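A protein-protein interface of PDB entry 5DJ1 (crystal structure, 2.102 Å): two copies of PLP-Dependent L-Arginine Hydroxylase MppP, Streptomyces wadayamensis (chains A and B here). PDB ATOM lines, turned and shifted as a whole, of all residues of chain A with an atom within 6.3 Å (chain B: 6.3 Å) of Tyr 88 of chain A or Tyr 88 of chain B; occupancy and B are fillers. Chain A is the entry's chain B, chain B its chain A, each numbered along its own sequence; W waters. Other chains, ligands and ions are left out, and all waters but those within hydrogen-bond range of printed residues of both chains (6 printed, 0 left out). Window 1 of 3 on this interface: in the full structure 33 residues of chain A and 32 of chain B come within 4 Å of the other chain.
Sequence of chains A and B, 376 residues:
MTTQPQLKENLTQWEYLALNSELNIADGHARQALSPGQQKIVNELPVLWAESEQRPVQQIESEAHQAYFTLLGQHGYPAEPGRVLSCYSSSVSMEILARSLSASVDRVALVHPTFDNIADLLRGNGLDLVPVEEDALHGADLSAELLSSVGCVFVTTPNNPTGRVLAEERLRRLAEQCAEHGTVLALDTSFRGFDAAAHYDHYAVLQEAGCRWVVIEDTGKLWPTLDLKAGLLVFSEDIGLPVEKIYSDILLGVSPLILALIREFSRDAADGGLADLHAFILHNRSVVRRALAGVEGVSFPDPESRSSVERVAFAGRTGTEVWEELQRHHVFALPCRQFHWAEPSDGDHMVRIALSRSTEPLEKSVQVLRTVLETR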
ATOM      1  N   SER A  86     -16.854  13.435  35.907  1.00  0.00           N
ATOM      2  CA  SER A  86     -16.864  12.836  34.580  1.00  0.00           C
ATOM      3  C   SER A  86     -18.249  12.929  33.959  1.00  0.00           C
ATOM      4  O   SER A  86     -19.230  12.488  34.564  1.00  0.00           O
ATOM      5  CB  SER A  86     -16.440  11.370  34.658  1.00  0.00           C
ATOM      6  OG  SER A  86     -15.110  11.241  35.114  1.00  0.00           O
ATOM      7  N   CYS A  87     -18.330  13.465  32.742  1.00  0.00           N
ATOM      8  CA  CYS A  87     -19.600  13.670  32.042  1.00  0.00           C
ATOM      9  C   CYS A  87     -19.594  12.927  30.710  1.00  0.00           C
ATOM     10  O   CYS A  87     -18.536  12.625  30.167  1.00  0.00           O
ATOM     11  CB  CYS A  87     -19.884  15.170  31.761  1.00  0.00           C
ATOM     12  SG  CYS A  87     -19.708  16.323  33.188  1.00  0.00           S
ATOM     13  N   TYR A  88     -20.799  12.662  30.169  1.00  0.00           N
ATOM     14  CA  TYR A  88     -20.919  11.906  28.904  1.00  0.00           C
ATOM     15  C   TYR A  88     -20.176  12.587  27.764  1.00  0.00           C
ATOM     16  O   TYR A  88     -19.705  11.933  26.834  1.00  0.00           O
ATOM     17  CB  TYR A  88     -22.402  11.750  28.525  1.00  0.00           C
ATOM     18  CG  TYR A  88     -23.247  11.042  29.552  1.00  0.00           C
ATOM     19  CD1 TYR A  88     -22.964   9.741  29.926  1.00  0.00           C
ATOM     20  CD2 TYR A  88     -24.361  11.675  30.124  1.00  0.00           C
ATOM     21  CE1 TYR A  88     -23.736   9.100  30.877  1.00  0.00           C
ATOM     22  CE2 TYR A  88     -25.143  11.049  31.043  1.00  0.00           C
ATOM     23  CZ  TYR A  88     -24.830   9.736  31.410  1.00  0.00           C
ATOM     24  OH  TYR A  88     -25.584   9.092  32.348  1.00  0.00           O
ATOM     25  N   SER A  89     -20.094  13.907  27.802  1.00  0.00           N
ATOM     26  CA  SER A  89     -19.385  14.658  26.788  1.00  0.00           C
ATOM     27  C   SER A  89     -19.029  16.018  27.366  1.00  0.00           C
ATOM     28  O   SER A  89     -19.562  16.445  28.393  1.00  0.00           O
ATOM     29  CB  SER A  89     -20.217  14.862  25.541  1.00  0.00           C
ATOM     30  OG  SER A  89     -21.281  15.750  25.809  1.00  0.00           O
ATOM     31  N   SER A  90     -18.195  16.731  26.615  1.00  0.00           N
ATOM     32  CA  SER A  90     -17.860  18.100  26.960  1.00  0.00           C
ATOM     33  C   SER A  90     -19.051  19.028  26.788  1.00  0.00           C
ATOM     34  O   SER A  90     -19.186  20.004  27.540  1.00  0.00           O
ATOM     35  CB  SER A  90     -16.685  18.542  26.094  1.00  0.00           C
ATOM     36  OG  SER A  90     -16.522  19.926  26.165  1.00  0.00           O
ATOM     37  N   SER A  91     -19.959  18.712  25.856  1.00  0.00           N
ATOM     38  CA  SER A  91     -21.159  19.548  25.705  1.00  0.00           C
ATOM     39  C   SER A  91     -22.146  19.363  26.856  1.00  0.00           C
ATOM     40  O   SER A  91     -22.829  20.333  27.237  1.00  0.00           O
ATOM     41  CB  SER A  91     -21.852  19.301  24.353  1.00  0.00           C
ATOM     42  OG  SER A  91     -21.028  19.733  23.257  1.00  0.00           O
ATOM     43  N   VAL A  92     -22.224  18.162  27.445  1.00  0.00           N
ATOM     44  CA  VAL A  92     -22.994  17.987  28.687  1.00  0.00           C
ATOM     45  C   VAL A  92     -22.348  18.778  29.832  1.00  0.00           C
ATOM     46  O   VAL A  92     -23.038  19.476  30.587  1.00  0.00           O
ATOM     47  CB  VAL A  92     -23.149  16.484  29.018  1.00  0.00           C
ATOM     48  CG1 VAL A  92     -23.805  16.241  30.423  1.00  0.00           C
ATOM     49  CG2 VAL A  92     -23.991  15.824  27.969  1.00  0.00           C
ATOM     50  N   SER A  93     -21.007  18.716  29.953  1.00  0.00           N
ATOM     51  CA  SER A  93     -20.296  19.569  30.904  1.00  0.00           C
ATOM     52  C   SER A  93     -20.660  21.037  30.700  1.00  0.00           C
ATOM     53  O   SER A  93     -20.908  21.775  31.669  1.00  0.00           O
ATOM     54  CB  SER A  93     -18.779  19.395  30.760  1.00  0.00           C
ATOM     55  OG  SER A  93     -18.406  18.032  30.864  1.00  0.00           O
ATOM     56  N1  LLP A 221     -15.566  22.158  22.729  1.00  0.00           N
ATOM     57  C2  LLP A 221     -14.861  22.306  21.592  1.00  0.00           C
ATOM     58  C2' LLP A 221     -14.015  23.524  21.364  1.00  0.00           C
ATOM     59  C3  LLP A 221     -14.892  21.251  20.576  1.00  0.00           C
ATOM     60  O3  LLP A 221     -14.175  21.397  19.440  1.00  0.00           O
ATOM     61  C4  LLP A 221     -15.716  20.057  20.831  1.00  0.00           C
ATOM     62  C4' LLP A 221     -15.685  18.956  19.867  1.00  0.00           C
ATOM     63  C5  LLP A 221     -16.439  20.008  22.120  1.00  0.00           C
ATOM     64  C6  LLP A 221     -16.322  21.093  22.989  1.00  0.00           C
ATOM     65  C5' LLP A 221     -17.309  18.840  22.575  1.00  0.00           C
ATOM     66  OP4 LLP A 221     -18.025  18.209  21.533  1.00  0.00           O
ATOM     67  P   LLP A 221     -19.002  16.978  21.831  1.00  0.00           P
ATOM     68  OP1 LLP A 221     -19.780  16.938  20.538  1.00  0.00           O
ATOM     69  OP2 LLP A 221     -18.139  15.763  22.049  1.00  0.00           O
ATOM     70  OP3 LLP A 221     -19.797  17.425  23.047  1.00  0.00           O
ATOM     71  N   LLP A 221     -11.992  14.527  21.015  1.00  0.00           N
ATOM     72  CA  LLP A 221     -11.453  14.960  19.726  1.00  0.00           C
ATOM     73  CB  LLP A 221     -11.312  16.502  19.692  1.00  0.00           C
ATOM     74  CG  LLP A 221     -12.651  17.241  19.604  1.00  0.00           C
ATOM     75  CD  LLP A 221     -13.216  17.261  18.184  1.00  0.00           C
ATOM     76  CE  LLP A 221     -14.649  17.810  18.074  1.00  0.00           C
ATOM     77  NZ  LLP A 221     -14.772  18.937  18.991  1.00  0.00           N
ATOM     78  C   LLP A 221     -10.137  14.271  19.382  1.00  0.00           C
ATOM     79  O   LLP A 221      -9.697  14.311  18.208  1.00  0.00           O
ATOM     80  N   ASP A 227     -16.955   8.049  19.237  1.00  0.00           N
ATOM     81  CA  ASP A 227     -17.629   8.927  20.195  1.00  0.00           C
ATOM     82  C   ASP A 227     -17.697   8.349  21.615  1.00  0.00           C
ATOM     83  O   ASP A 227     -18.497   8.798  22.425  1.00  0.00           O
ATOM     84  CB  ASP A 227     -19.032   9.296  19.702  1.00  0.00           C
ATOM     85  CG  ASP A 227     -19.026  10.559  18.860  1.00  0.00           C
ATOM     86  OD1 ASP A 227     -18.628  11.615  19.395  1.00  0.00           O
ATOM     87  OD2 ASP A 227     -19.399  10.499  17.669  1.00  0.00           O
ATOM     88  N   LYS A 229     -16.271   8.649  24.944  1.00  0.00           N
ATOM     89  CA  LYS A 229     -15.492   9.794  25.388  1.00  0.00           C
ATOM     90  C   LYS A 229     -16.006  10.252  26.746  1.00  0.00           C
ATOM     91  O   LYS A 229     -16.993   9.734  27.272  1.00  0.00           O
ATOM     92  CB  LYS A 229     -15.579  10.926  24.353  1.00  0.00           C
ATOM     93  CG  LYS A 229     -17.050  11.445  24.207  1.00  0.00           C
ATOM     94  CD  LYS A 229     -17.239  12.233  22.916  1.00  0.00           C
ATOM     95  CE  LYS A 229     -18.739  12.507  22.673  1.00  0.00           C
ATOM     96  NZ  LYS A 229     -18.969  13.357  21.460  1.00  0.00           N
ATOM     97  N   ALA A 230     -15.338  11.262  27.295  1.00  0.00           N
ATOM     98  CA  ALA A 230     -15.819  11.941  28.484  1.00  0.00           C
ATOM     99  C   ALA A 230     -15.437  13.405  28.436  1.00  0.00           C
ATOM    100  O   ALA A 230     -14.334  13.758  27.994  1.00  0.00           O
ATOM    101  CB  ALA A 230     -15.255  11.312  29.758  1.00  0.00           C
ATOM    102  N   GLY A 231     -16.355  14.248  28.906  1.00  0.00           N
ATOM    103  CA  GLY A 231     -15.999  15.578  29.340  1.00  0.00           C
ATOM    104  C   GLY A 231     -15.610  15.494  30.806  1.00  0.00           C
ATOM    105  O   GLY A 231     -16.243  14.791  31.590  1.00  0.00           O
ATOM    106  N   ILE A 250     -28.179  15.564  36.527  1.00  0.00           N
ATOM    107  CA  ILE A 250     -28.121  14.994  35.188  1.00  0.00           C
ATOM    108  C   ILE A 250     -27.485  13.593  35.174  1.00  0.00           C
ATOM    109  O   ILE A 250     -27.893  12.744  34.372  1.00  0.00           O
ATOM    110  CB  ILE A 250     -27.392  15.971  34.240  1.00  0.00           C
ATOM    111  CG1 ILE A 250     -28.251  17.232  34.076  1.00  0.00           C
ATOM    112  CG2 ILE A 250     -27.098  15.292  32.870  1.00  0.00           C
ATOM    113  CD1 ILE A 250     -27.667  18.288  33.225  1.00  0.00           C
ATOM    114  N   LEU A 251     -26.466  13.284  35.994  1.00  0.00           N
ATOM    115  CA  LEU A 251     -25.905  11.936  35.905  1.00  0.00           C
ATOM    116  C   LEU A 251     -25.183  11.552  37.186  1.00  0.00           C
ATOM    117  O   LEU A 251     -24.751  12.399  37.961  1.00  0.00           O
ATOM    118  CB  LEU A 251     -24.944  11.789  34.709  1.00  0.00           C
ATOM    119  CG  LEU A 251     -23.593  12.549  34.718  1.00  0.00           C
ATOM    120  CD1 LEU A 251     -22.625  11.871  33.732  1.00  0.00           C
ATOM    121  CD2 LEU A 251     -23.755  14.027  34.370  1.00  0.00           C
ATOM    122  N   LEU A 252     -25.048  10.248  37.380  1.00  0.00           N
ATOM    123  CA  LEU A 252     -24.267   9.715  38.486  1.00  0.00           C
ATOM    124  C   LEU A 252     -22.806   9.542  38.117  1.00  0.00           C
ATOM    125  O   LEU A 252     -21.946   9.526  39.001  1.00  0.00           O
ATOM    126  CB  LEU A 252     -24.803   8.351  38.904  1.00  0.00           C
ATOM    127  CG  LEU A 252     -26.205   8.243  39.500  1.00  0.00           C
ATOM    128  CD1 LEU A 252     -26.615   6.767  39.528  1.00  0.00           C
ATOM    129  CD2 LEU A 252     -26.266   8.864  40.902  1.00  0.00           C
ATOM    130  N   GLY A 253     -22.517   9.410  36.836  1.00  0.00           N
ATOM    131  CA  GLY A 253     -21.163   9.204  36.376  1.00  0.00           C
ATOM    132  C   GLY A 253     -21.207   8.547  35.016  1.00  0.00           C
ATOM    133  O   GLY A 253     -22.266   8.287  34.466  1.00  0.00           O
ATOM    134  N   VAL A 254     -20.018   8.264  34.508  1.00  0.00           N
ATOM    135  CA  VAL A 254     -19.819   7.688  33.197  1.00  0.00           C
ATOM    136  C   VAL A 254     -19.473   6.200  33.333  1.00  0.00           C
ATOM    137  O   VAL A 254     -19.003   5.728  34.377  1.00  0.00           O
ATOM    138  CB  VAL A 254     -18.720   8.523  32.501  1.00  0.00           C
ATOM    139  CG1 VAL A 254     -18.066   7.828  31.373  1.00  0.00           C
ATOM    140  CG2 VAL A 254     -19.374   9.856  32.043  1.00  0.00           C
ATOM    141  N   SER A 255     -19.740   5.445  32.266  1.00  0.00           N
ATOM    142  CA  SER A 255     -19.508   4.017  32.248  1.00  0.00           C
ATOM    143  C   SER A 255     -18.069   3.713  32.655  1.00  0.00           C
ATOM    144  O   SER A 255     -17.140   4.351  32.128  1.00  0.00           O
ATOM    145  CB  SER A 255     -19.758   3.446  30.852  1.00  0.00           C
ATOM    146  OG  SER A 255     -19.306   2.094  30.762  1.00  0.00           O
ATOM    147  N   SER B  86     -31.627   9.908  19.708  1.00  0.00           N
ATOM    148  CA  SER B  86     -30.839   9.125  20.654  1.00  0.00           C
ATOM    149  C   SER B  86     -29.987  10.037  21.530  1.00  0.00           C
ATOM    150  O   SER B  86     -29.191  10.828  21.023  1.00  0.00           O
ATOM    151  CB  SER B  86     -29.939   8.129  19.912  1.00  0.00           C
ATOM    152  OG  SER B  86     -30.717   7.285  19.075  1.00  0.00           O
ATOM    153  N   CYS B  87     -30.113   9.886  22.836  1.00  0.00           N
ATOM    154  CA  CYS B  87     -29.361  10.668  23.814  1.00  0.00           C
ATOM    155  C   CYS B  87     -28.470   9.774  24.679  1.00  0.00           C
ATOM    156  O   CYS B  87     -28.731   8.580  24.849  1.00  0.00           O
ATOM    157  CB  CYS B  87     -30.316  11.464  24.734  1.00  0.00           C
ATOM    158  SG  CYS B  87     -31.590  12.464  23.820  1.00  0.00           S
ATOM    159  N   TYR B  88     -27.445  10.394  25.286  1.00  0.00           N
ATOM    160  CA  TYR B  88     -26.511   9.662  26.152  1.00  0.00           C
ATOM    161  C   TYR B  88     -27.219   8.968  27.303  1.00  0.00           C
ATOM    162  O   TYR B  88     -26.756   7.930  27.788  1.00  0.00           O
ATOM    163  CB  TYR B  88     -25.464  10.617  26.742  1.00  0.00           C
ATOM    164  CG  TYR B  88     -24.597  11.311  25.731  1.00  0.00           C
ATOM    165  CD1 TYR B  88     -23.834  10.598  24.818  1.00  0.00           C
ATOM    166  CD2 TYR B  88     -24.548  12.694  25.686  1.00  0.00           C
ATOM    167  CE1 TYR B  88     -23.028  11.249  23.893  1.00  0.00           C
ATOM    168  CE2 TYR B  88     -23.763  13.349  24.755  1.00  0.00           C
ATOM    169  CZ  TYR B  88     -23.006  12.624  23.868  1.00  0.00           C
ATOM    170  OH  TYR B  88     -22.235  13.306  22.952  1.00  0.00           O
ATOM    171  N   SER B  89     -28.333   9.530  27.765  1.00  0.00           N
ATOM    172  CA  SER B  89     -29.082   8.953  28.861  1.00  0.00           C
ATOM    173  C   SER B  89     -30.481   9.532  28.837  1.00  0.00           C
ATOM    174  O   SER B  89     -30.747  10.543  28.187  1.00  0.00           O
ATOM    175  CB  SER B  89     -28.429   9.256  30.207  1.00  0.00           C
ATOM    176  OG  SER B  89     -28.651  10.612  30.520  1.00  0.00           O
ATOM    177  N   SER B  90     -31.358   8.901  29.618  1.00  0.00           N
ATOM    178  CA  SER B  90     -32.719   9.416  29.810  1.00  0.00           C
ATOM    179  C   SER B  90     -32.723  10.758  30.532  1.00  0.00           C
ATOM    180  O   SER B  90     -33.589  11.612  30.257  1.00  0.00           O
ATOM    181  CB  SER B  90     -33.556   8.385  30.584  1.00  0.00           C
ATOM    182  OG  SER B  90     -34.793   8.940  31.002  1.00  0.00           O
ATOM    183  N   SER B  91     -31.776  10.977  31.454  1.00  0.00           N
ATOM    184  CA  SER B  91     -31.721  12.259  32.143  1.00  0.00           C
ATOM    185  C   SER B  91     -31.226  13.356  31.212  1.00  0.00           C
ATOM    186  O   SER B  91     -31.647  14.503  31.355  1.00  0.00           O
ATOM    187  CB  SER B  91     -30.826  12.175  33.403  1.00  0.00           C
ATOM    188  OG  SER B  91     -31.403  11.307  34.385  1.00  0.00           O
ATOM    189  N   VAL B  92     -30.345  13.037  30.244  1.00  0.00           N
ATOM    190  CA  VAL B  92     -29.994  14.036  29.230  1.00  0.00           C
ATOM    191  C   VAL B  92     -31.216  14.395  28.389  1.00  0.00           C
ATOM    192  O   VAL B  92     -31.456  15.573  28.107  1.00  0.00           O
ATOM    193  CB  VAL B  92     -28.819  13.559  28.356  1.00  0.00           C
ATOM    194  CG1 VAL B  92     -28.620  14.498  27.157  1.00  0.00           C
ATOM    195  CG2 VAL B  92     -27.525  13.554  29.194  1.00  0.00           C
ATOM    196  N   SER B  93     -31.999  13.383  27.969  1.00  0.00           N
ATOM    197  CA  SER B  93     -33.269  13.637  27.283  1.00  0.00           C
ATOM    198  C   SER B  93     -34.174  14.517  28.124  1.00  0.00           C
ATOM    199  O   SER B  93     -34.840  15.421  27.615  1.00  0.00           O
ATOM    200  CB  SER B  93     -34.016  12.329  26.982  1.00  0.00           C
ATOM    201  OG  SER B  93     -33.202  11.409  26.265  1.00  0.00           O
ATOM    202  N1  LLP B 221     -36.282   7.904  34.517  1.00  0.00           N
ATOM    203  C2  LLP B 221     -36.565   6.942  35.411  1.00  0.00           C
ATOM    204  C2' LLP B 221     -37.965   6.689  35.874  1.00  0.00           C
ATOM    205  C3  LLP B 221     -35.491   6.092  35.944  1.00  0.00           C
ATOM    206  O3  LLP B 221     -35.764   5.116  36.823  1.00  0.00           O
ATOM    207  C4  LLP B 221     -34.113   6.338  35.518  1.00  0.00           C
ATOM    208  C4' LLP B 221     -33.015   5.461  35.967  1.00  0.00           C
ATOM    209  C5  LLP B 221     -33.935   7.433  34.544  1.00  0.00           C
ATOM    210  C6  LLP B 221     -35.036   8.159  34.108  1.00  0.00           C
ATOM    211  C5' LLP B 221     -32.587   7.756  33.928  1.00  0.00           C
ATOM    212  OP4 LLP B 221     -31.463   7.504  34.701  1.00  0.00           O
ATOM    213  P   LLP B 221     -29.983   7.801  34.159  1.00  0.00           P
ATOM    214  OP1 LLP B 221     -30.076   9.104  33.369  1.00  0.00           O
ATOM    215  OP2 LLP B 221     -29.195   7.933  35.446  1.00  0.00           O
ATOM    216  OP3 LLP B 221     -29.515   6.669  33.261  1.00  0.00           O
ATOM    217  N   LLP B 221     -31.897   0.822  32.542  1.00  0.00           N
ATOM    218  CA  LLP B 221     -32.236   0.115  33.782  1.00  0.00           C
ATOM    219  CB  LLP B 221     -33.478   0.728  34.436  1.00  0.00           C
ATOM    220  CG  LLP B 221     -33.236   2.147  34.978  1.00  0.00           C
ATOM    221  CD  LLP B 221     -32.653   2.128  36.388  1.00  0.00           C
ATOM    222  CE  LLP B 221     -32.206   3.490  36.918  1.00  0.00           C
ATOM    223  NZ  LLP B 221     -33.290   4.406  36.576  1.00  0.00           N
ATOM    224  C   LLP B 221     -32.418  -1.371  33.570  1.00  0.00           C
ATOM    225  O   LLP B 221     -32.453  -2.153  34.540  1.00  0.00           O
ATOM    226  N   ASP B 227     -23.656   0.890  32.468  1.00  0.00           N
ATOM    227  CA  ASP B 227     -24.176   2.220  32.102  1.00  0.00           C
ATOM    228  C   ASP B 227     -23.926   2.603  30.656  1.00  0.00           C
ATOM    229  O   ASP B 227     -24.004   3.781  30.297  1.00  0.00           O
ATOM    230  CB  ASP B 227     -23.647   3.290  33.057  1.00  0.00           C
ATOM    231  CG  ASP B 227     -24.575   3.456  34.233  1.00  0.00           C
ATOM    232  OD1 ASP B 227     -25.663   4.068  34.031  1.00  0.00           O
ATOM    233  OD2 ASP B 227     -24.272   2.898  35.314  1.00  0.00           O
ATOM    234  N   LYS B 229     -25.725   2.876  27.426  1.00  0.00           N
ATOM    235  CA  LYS B 229     -27.171   3.060  27.357  1.00  0.00           C
ATOM    236  C   LYS B 229     -27.482   4.225  26.431  1.00  0.00           C
ATOM    237  O   LYS B 229     -26.601   4.994  26.032  1.00  0.00           O
ATOM    238  CB  LYS B 229     -27.759   3.323  28.746  1.00  0.00           C
ATOM    239  CG  LYS B 229     -27.205   4.574  29.398  1.00  0.00           C
ATOM    240  CD  LYS B 229     -27.484   4.688  30.861  1.00  0.00           C
ATOM    241  CE  LYS B 229     -26.749   5.912  31.401  1.00  0.00           C
ATOM    242  NZ  LYS B 229     -26.919   6.132  32.854  1.00  0.00           N
ATOM    243  N   ALA B 230     -28.766   4.359  26.121  1.00  0.00           N
ATOM    244  CA  ALA B 230     -29.282   5.534  25.457  1.00  0.00           C
ATOM    245  C   ALA B 230     -30.627   5.919  26.054  1.00  0.00           C
ATOM    246  O   ALA B 230     -31.405   5.047  26.443  1.00  0.00           O
ATOM    247  CB  ALA B 230     -29.432   5.291  23.964  1.00  0.00           C
ATOM    248  N   GLY B 231     -30.880   7.227  26.152  1.00  0.00           N
ATOM    249  CA  GLY B 231     -32.237   7.732  26.289  1.00  0.00           C
ATOM    250  C   GLY B 231     -32.773   7.989  24.887  1.00  0.00           C
ATOM    251  O   GLY B 231     -32.038   8.409  23.999  1.00  0.00           O
ATOM    252  N   ILE B 250     -26.688  20.021  22.474  1.00  0.00           N
ATOM    253  CA  ILE B 250     -26.033  19.158  23.456  1.00  0.00           C
ATOM    254  C   ILE B 250     -25.248  18.006  22.791  1.00  0.00           C
ATOM    255  O   ILE B 250     -24.152  17.667  23.247  1.00  0.00           O
ATOM    256  CB  ILE B 250     -27.094  18.664  24.468  1.00  0.00           C
ATOM    257  CG1 ILE B 250     -27.584  19.877  25.310  1.00  0.00           C
ATOM    258  CG2 ILE B 250     -26.542  17.535  25.412  1.00  0.00           C
ATOM    259  CD1 ILE B 250     -28.698  19.597  26.236  1.00  0.00           C
ATOM    260  N   LEU B 251     -25.748  17.397  21.706  1.00  0.00           N
ATOM    261  CA  LEU B 251     -25.042  16.304  21.032  1.00  0.00           C
ATOM    262  C   LEU B 251     -25.525  16.129  19.592  1.00  0.00           C
ATOM    263  O   LEU B 251     -26.641  16.513  19.233  1.00  0.00           O
ATOM    264  CB  LEU B 251     -25.216  14.966  21.759  1.00  0.00           C
ATOM    265  CG  LEU B 251     -26.583  14.270  21.744  1.00  0.00           C
ATOM    266  CD1 LEU B 251     -26.450  12.810  22.198  1.00  0.00           C
ATOM    267  CD2 LEU B 251     -27.534  14.991  22.643  1.00  0.00           C
ATOM    268  N   LEU B 252     -24.674  15.489  18.797  1.00  0.00           N
ATOM    269  CA  LEU B 252     -24.973  15.033  17.446  1.00  0.00           C
ATOM    270  C   LEU B 252     -25.606  13.647  17.415  1.00  0.00           C
ATOM    271  O   LEU B 252     -26.317  13.316  16.462  1.00  0.00           O
ATOM    272  CB  LEU B 252     -23.682  14.981  16.624  1.00  0.00           C
ATOM    273  CG  LEU B 252     -22.855  16.259  16.464  1.00  0.00           C
ATOM    274  CD1 LEU B 252     -21.430  15.937  15.989  1.00  0.00           C
ATOM    275  CD2 LEU B 252     -23.544  17.202  15.496  1.00  0.00           C
ATOM    276  N   GLY B 253     -25.335  12.837  18.426  1.00  0.00           N
ATOM    277  CA  GLY B 253     -25.799  11.465  18.489  1.00  0.00           C
ATOM    278  C   GLY B 253     -24.973  10.698  19.500  1.00  0.00           C
ATOM    279  O   GLY B 253     -24.060  11.238  20.127  1.00  0.00           O
ATOM    280  N   VAL B 254     -25.314   9.423  19.655  1.00  0.00           N
ATOM    281  CA  VAL B 254     -24.586   8.530  20.563  1.00  0.00           C
ATOM    282  C   VAL B 254     -23.684   7.591  19.762  1.00  0.00           C
ATOM    283  O   VAL B 254     -23.882   7.357  18.568  1.00  0.00           O
ATOM    284  CB  VAL B 254     -25.538   7.709  21.461  1.00  0.00           C
ATOM    285  CG1 VAL B 254     -26.406   8.629  22.302  1.00  0.00           C
ATOM    286  CG2 VAL B 254     -26.387   6.778  20.632  1.00  0.00           C
ATOM    287  N   SER B 255     -22.707   7.004  20.456  1.00  0.00           N
ATOM    288  CA  SER B 255     -21.762   6.086  19.844  1.00  0.00           C
ATOM    289  C   SER B 255     -22.497   4.982  19.075  1.00  0.00           C
ATOM    290  O   SER B 255     -23.431   4.363  19.617  1.00  0.00           O
ATOM    291  CB  SER B 255     -20.864   5.450  20.896  1.00  0.00           C
ATOM    292  OG  SER B 255     -20.041   4.448  20.301  1.00  0.00           O
HETATM  293  O   HOH W   1     -21.507  12.348  20.075  1.00  0.00           O
HETATM  294  O   HOH W   2     -24.519   6.951  34.420  1.00  0.00           O
HETATM  295  O   HOH W   3     -26.633   8.354  35.655  1.00  0.00           O
HETATM  296  O   HOH W   4     -21.826  15.207  19.832  1.00  0.00           O
HETATM  297  O   HOH W   5     -27.712  10.453  33.106  1.00  0.00           O
HETATM  298  O   HOH W   6     -22.233  15.973  23.234  1.00  0.00           O
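NZ of Lys 229 of chain B is in hydrogen-bond range of OH of Tyr 88 of chain A (3.3 Å).
The side-chain hydroxyl (OG) of Ser 91 of chain B lies within hydrogen-bond range of OP1 of LLP 221 of chain B.
OG of Ser 89 of chain B sits close to N of Ser 91 of chain B.
NZ of Lys 229 of chain B is in salt-bridge range of OD1 of Asp 227 of chain B (2.7 Å).
The side-chain hydroxyl of Ser 91 of chain A is in hydrogen-bond range of OP3 of LLP 221 of chain A.
The backbone carbonyl oxygen (O) of Ser 89 of chain B sits at hydrogen-bond distance from the side-chain hydroxyl (OG) of Ser 93 of chain B (3.2 Å).
Among the printed residues, pairs that only touch across the chains: Ser 91 of chain A with Ile 250 of chain B, Ile 250 of chain A with Ser 91 of chain B, Tyr 88 of chain A with Ser 89 of chain B, Tyr 88 of chain A with Tyr 88 of chain B, Lys 229 of chain A with Tyr 88 of chain B, Ser 89 of chain A with Tyr 88 of chain B, Tyr 88 of chain A with Val 92 of chain B, Val 92 of chain A with Tyr 88 of chain B and Val 92 of chain A with Ile 250 of chain B.
Of chain B, only Tyr 88 (3.6 Å), Ser 89 (3.6 Å), Val 92 (3.8 Å) and Lys 229 (3.3 Å) come within 4 Å of Tyr 88 of chain A.
Printed residues of chain B within 4 Å of Val 92 of chain A: Tyr 88 and Ile 250.
Asp 227 of chain A touches none of the printed residues of chain B.
Printed residues of chain B within 4 Å of Lys 229 of chain A: Tyr 88 (3.6 Å).
Of chain A, only Tyr 88, Ser 89, Val 92 and Lys 229 come within 4 Å of Tyr 88 of chain B.
Of the printed residues of chain A, Ser 89 of chain B touches Tyr 88.
Of the printed residues of chain A, Ser 91 of chain B touches Ile 250 (3.1 Å).
Of the printed residues of chain A, Ile 250 of chain B touches Ser 91 (3.0 Å) and Val 92 (3.997 Å).
The nearest residue of chain A that does not touch Tyr 88 of chain B is LLP 221 of chain A (4.8 Å).
Hydrophobic or aromatic side chains of chain A within 4 Å of the printed part of chain B: Tyr 88 and Val 92.
Printed residues of chain B that touch a printed residue of chain A: Tyr 88, Ser 89, Ser 91, Val 92, Lys 229 and Ile 250.
Along chain B the printed residues that touch a printed residue of chain A span positions 88 to 250.
Among the printed residues, 10 pairs touch across the chains.
Tyr 88 of chain B touches its own counterpart, Tyr 88 of chain A.
Tyr 88 of chain A touches Val 92 of chain B, and with the chains exchanged Val 92 of chain A touches Tyr 88 of chain B.
Tyr 88 of chain A touches Lys 229 of chain B, and with the chains exchanged Lys 229 of chain A touches Tyr 88 of chain B.
Ser 91 of chain A touches Ile 250 of chain B, and with the chains exchanged Ile 250 of chain A touches Ser 91 of chain B.
Water W5 lies within hydrogen-bond range of the backbone carbonyl oxygen of Ile 250 of chain A, the side-chain hydroxyl of Tyr 88 of chain A, OP1 of LLP 221 of chain B and the side-chain hydroxyl of Ser 89 of chain B.
Water W1 lies within hydrogen-bond range of O of Gly 253 of chain B (2.8 Å), OD1 of Asp 227 of chain A (3.0 Å), NZ of Lys 229 of chain A (3.1 Å) and OH of Tyr 88 of chain B (3.1 Å).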
